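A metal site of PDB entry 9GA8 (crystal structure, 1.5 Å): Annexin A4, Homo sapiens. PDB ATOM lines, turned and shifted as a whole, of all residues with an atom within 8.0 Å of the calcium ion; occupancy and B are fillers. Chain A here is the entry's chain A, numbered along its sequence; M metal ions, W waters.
The side-chain hydroxyl (OG1) of Thr 32 sits close to the side-chain carboxylate (OE1) of Glu 71.
The nearest printed residue that does not touch the calcium ion is Leu 30 (4.1 Å).
The calcium ion is bound by O of Met 27 (2.3 Å), water W1 (2.3 Å), O of Gly 29 (2.4 Å), water W2 (2.4 Å), OE2 of Glu 71 (2.4 Å), O of Gly 31 (2.5 Å) and OE1 of Glu 71 (2.6 Å). The calcium ion has seven donor atoms within binding distance.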
ATOM      1  N   ARG A  24      -3.081 -18.195 -19.921  1.00  0.00           N
ATOM      2  CA  ARG A  24      -4.010 -17.563 -19.006  1.00  0.00           C
ATOM      3  C   ARG A  24      -5.237 -17.120 -19.810  1.00  0.00           C
ATOM      4  O   ARG A  24      -6.365 -17.280 -19.361  1.00  0.00           O
ATOM      5  CB  ARG A  24      -3.376 -16.349 -18.350  1.00  0.00           C
ATOM      6  CG  ARG A  24      -4.300 -15.454 -17.529  1.00  0.00           C
ATOM      7  CD  ARG A  24      -5.091 -16.202 -16.503  1.00  0.00           C
ATOM      8  NE  ARG A  24      -5.776 -15.231 -15.638  1.00  0.00           N
ATOM      9  CZ  ARG A  24      -6.800 -15.492 -14.875  1.00  0.00           C
ATOM     10  NH1 ARG A  24      -7.285 -16.723 -14.760  1.00  0.00           N
ATOM     11  NH2 ARG A  24      -7.405 -14.459 -14.310  1.00  0.00           N
ATOM     12  N   LYS A  25      -5.044 -16.490 -20.961  1.00  0.00           N
ATOM     13  CA  LYS A  25      -6.177 -16.092 -21.802  1.00  0.00           C
ATOM     14  C   LYS A  25      -7.074 -17.259 -22.158  1.00  0.00           C
ATOM     15  O   LYS A  25      -8.322 -17.133 -22.146  1.00  0.00           O
ATOM     16  CB  LYS A  25      -5.700 -15.437 -23.106  1.00  0.00           C
ATOM     17  CG  LYS A  25      -5.206 -14.032 -22.902  1.00  0.00           C
ATOM     18  CD  LYS A  25      -6.283 -12.958 -23.016  1.00  0.00           C
ATOM     19  CE  LYS A  25      -5.707 -11.584 -23.136  1.00  0.00           C
ATOM     20  NZ  LYS A  25      -5.101 -11.191 -21.868  1.00  0.00           N
ATOM     21  N   ALA A  26      -6.456 -18.423 -22.406  1.00  0.00           N
ATOM     22  CA  ALA A  26      -7.198 -19.619 -22.734  1.00  0.00           C
ATOM     23  C   ALA A  26      -8.096 -20.058 -21.570  1.00  0.00           C
ATOM     24  O   ALA A  26      -9.140 -20.663 -21.840  1.00  0.00           O
ATOM     25  CB  ALA A  26      -6.253 -20.728 -23.178  1.00  0.00           C
ATOM     26  N   MET A  27      -7.662 -19.870 -20.326  1.00  0.00           N
ATOM     27  CA  MET A  27      -8.397 -20.371 -19.166  1.00  0.00           C
ATOM     28  C   MET A  27      -9.272 -19.316 -18.491  1.00  0.00           C
ATOM     29  O   MET A  27     -10.237 -19.696 -17.846  1.00  0.00           O
ATOM     30  CB  MET A  27      -7.423 -21.024 -18.179  1.00  0.00           C
ATOM     31  CG  MET A  27      -6.697 -22.160 -18.782  1.00  0.00           C
ATOM     32  SD  MET A  27      -5.647 -23.069 -17.644  1.00  0.00           S
ATOM     33  CE  MET A  27      -4.203 -22.021 -17.871  1.00  0.00           C
ATOM     34  N   LYS A  28      -8.885 -18.047 -18.533  1.00  0.00           N
ATOM     35  CA  LYS A  28      -9.603 -17.052 -17.761  1.00  0.00           C
ATOM     36  C   LYS A  28     -11.077 -16.978 -18.190  1.00  0.00           C
ATOM     37  O   LYS A  28     -11.358 -16.862 -19.351  1.00  0.00           O
ATOM     38  CB  LYS A  28      -9.014 -15.678 -18.054  1.00  0.00           C
ATOM     39  CG  LYS A  28      -9.536 -14.604 -17.079  1.00  0.00           C
ATOM     40  CD  LYS A  28      -8.893 -13.263 -17.364  1.00  0.00           C
ATOM     41  CE  LYS A  28      -9.656 -12.147 -16.713  1.00  0.00           C
ATOM     42  NZ  LYS A  28      -8.838 -10.933 -16.715  1.00  0.00           N
ATOM     43  N   GLY A  29     -11.966 -16.859 -17.203  1.00  0.00           N
ATOM     44  CA  GLY A  29     -13.373 -16.723 -17.523  1.00  0.00           C
ATOM     45  C   GLY A  29     -14.056 -18.076 -17.706  1.00  0.00           C
ATOM     46  O   GLY A  29     -13.417 -19.118 -17.807  1.00  0.00           O
ATOM     47  N   LEU A  30     -15.399 -18.097 -17.810  1.00  0.00           N
ATOM     48  CA  LEU A  30     -16.092 -19.360 -17.989  1.00  0.00           C
ATOM     49  C   LEU A  30     -15.544 -20.028 -19.228  1.00  0.00           C
ATOM     50  O   LEU A  30     -15.266 -19.338 -20.229  1.00  0.00           O
ATOM     51  CB  LEU A  30     -17.604 -19.103 -18.139  1.00  0.00           C
ATOM     52  CG  LEU A  30     -18.459 -20.348 -18.430  1.00  0.00           C
ATOM     53  CD1 LEU A  30     -18.376 -21.579 -17.477  1.00  0.00           C
ATOM     54  CD2 LEU A  30     -19.952 -19.937 -18.502  1.00  0.00           C
ATOM     55  N   GLY A  31     -15.417 -21.345 -19.168  1.00  0.00           N
ATOM     56  CA  GLY A  31     -14.959 -22.152 -20.296  1.00  0.00           C
ATOM     57  C   GLY A  31     -13.424 -22.125 -20.422  1.00  0.00           C
ATOM     58  O   GLY A  31     -12.720 -21.517 -19.640  1.00  0.00           O
ATOM     59  N   THR A  32     -12.970 -22.772 -21.478  1.00  0.00           N
ATOM     60  CA  THR A  32     -11.545 -22.959 -21.746  1.00  0.00           C
ATOM     61  C   THR A  32     -11.370 -22.984 -23.251  1.00  0.00           C
ATOM     62  O   THR A  32     -12.240 -23.464 -23.980  1.00  0.00           O
ATOM     63  CB  THR A  32     -11.096 -24.290 -21.136  1.00  0.00           C
ATOM     64  OG1 THR A  32     -11.533 -24.429 -19.797  1.00  0.00           O
ATOM     65  CG2 THR A  32      -9.590 -24.438 -21.243  1.00  0.00           C
ATOM     66  N   ASP A  33     -10.273 -22.399 -23.762  1.00  0.00           N
ATOM     67  CA  ASP A  33      -9.831 -22.648 -25.114  1.00  0.00           C
ATOM     68  C   ASP A  33      -8.794 -23.781 -25.111  1.00  0.00           C
ATOM     69  O   ASP A  33      -7.593 -23.549 -25.053  1.00  0.00           O
ATOM     70  CB  ASP A  33      -9.319 -21.353 -25.719  1.00  0.00           C
ATOM     71  CG  ASP A  33      -8.892 -21.473 -27.166  1.00  0.00           C
ATOM     72  OD1 ASP A  33      -8.952 -22.601 -27.690  1.00  0.00           O
ATOM     73  OD2 ASP A  33      -8.497 -20.439 -27.720  1.00  0.00           O
ATOM     74  N   ARG A  62      -0.156 -16.595 -10.825  1.00  0.00           N
ATOM     75  CA  ARG A  62      -0.941 -17.797 -10.598  1.00  0.00           C
ATOM     76  C   ARG A  62      -0.068 -19.015 -10.786  1.00  0.00           C
ATOM     77  O   ARG A  62       1.047 -18.925 -11.297  1.00  0.00           O
ATOM     78  CB  ARG A  62      -2.150 -17.766 -11.549  1.00  0.00           C
ATOM     79  CG  ARG A  62      -3.102 -16.609 -11.361  1.00  0.00           C
ATOM     80  CD  ARG A  62      -4.274 -16.691 -12.357  1.00  0.00           C
ATOM     81  NE  ARG A  62      -5.117 -17.879 -12.206  1.00  0.00           N
ATOM     82  CZ  ARG A  62      -6.332 -17.874 -11.651  1.00  0.00           C
ATOM     83  NH1 ARG A  62      -6.830 -16.767 -11.168  1.00  0.00           N
ATOM     84  NH2 ARG A  62      -7.005 -18.982 -11.502  1.00  0.00           N
ATOM     85  N   ASP A  67      -4.055 -24.321 -12.308  1.00  0.00           N
ATOM     86  CA  ASP A  67      -5.047 -23.823 -13.217  1.00  0.00           C
ATOM     87  C   ASP A  67      -5.450 -24.927 -14.190  1.00  0.00           C
ATOM     88  O   ASP A  67      -6.603 -25.046 -14.524  1.00  0.00           O
ATOM     89  CB  ASP A  67      -4.627 -22.527 -13.887  1.00  0.00           C
ATOM     90  CG  ASP A  67      -4.673 -21.281 -13.049  1.00  0.00           C
ATOM     91  OD1 ASP A  67      -5.127 -21.391 -11.870  1.00  0.00           O
ATOM     92  OD2 ASP A  67      -4.258 -20.223 -13.587  1.00  0.00           O
ATOM     93  N   SER A  70      -7.670 -27.415 -12.567  1.00  0.00           N
ATOM     94  CA  SER A  70      -8.983 -26.844 -12.345  1.00  0.00           C
ATOM     95  C   SER A  70      -9.817 -26.789 -13.621  1.00  0.00           C
ATOM     96  O   SER A  70     -11.039 -27.037 -13.618  1.00  0.00           O
ATOM     97  CB  SER A  70      -8.799 -25.479 -11.748  1.00  0.00           C
ATOM     98  OG  SER A  70     -10.079 -24.955 -11.443  1.00  0.00           O
ATOM     99  N   GLU A  71      -9.183 -26.460 -14.757  1.00  0.00           N
ATOM    100  CA  GLU A  71      -9.941 -26.182 -15.946  1.00  0.00           C
ATOM    101  C   GLU A  71     -10.266 -27.456 -16.731  1.00  0.00           C
ATOM    102  O   GLU A  71     -11.228 -27.528 -17.444  1.00  0.00           O
ATOM    103  CB  GLU A  71      -9.060 -25.294 -16.832  1.00  0.00           C
ATOM    104  CG  GLU A  71      -8.942 -23.867 -16.332  1.00  0.00           C
ATOM    105  CD  GLU A  71     -10.096 -22.946 -16.705  1.00  0.00           C
ATOM    106  OE1 GLU A  71     -10.543 -22.979 -17.833  1.00  0.00           O
ATOM    107  OE2 GLU A  71     -10.467 -22.100 -15.832  1.00  0.00           O
ATOM    108  N   LEU A  72      -9.378 -28.430 -16.689  1.00  0.00           N
ATOM    109  CA  LEU A  72      -9.423 -29.555 -17.607  1.00  0.00           C
ATOM    110  C   LEU A  72      -9.939 -30.772 -16.862  1.00  0.00           C
ATOM    111  O   LEU A  72      -9.916 -30.758 -15.635  1.00  0.00           O
ATOM    112  CB  LEU A  72      -8.019 -29.839 -18.139  1.00  0.00           C
ATOM    113  CG  LEU A  72      -7.354 -28.698 -18.900  1.00  0.00           C
ATOM    114  CD1 LEU A  72      -6.060 -29.231 -19.534  1.00  0.00           C
ATOM    115  CD2 LEU A  72      -8.282 -28.142 -19.978  1.00  0.00           C
HETATM  116 CA    CA M   1     -12.069 -20.995 -17.313  1.00  0.00          CA
HETATM  117  O   HOH W   1     -13.761 -22.508 -16.747  1.00  0.00           O
HETATM  118  O   HOH W   2     -12.374 -19.960 -15.154  1.00  0.00           O
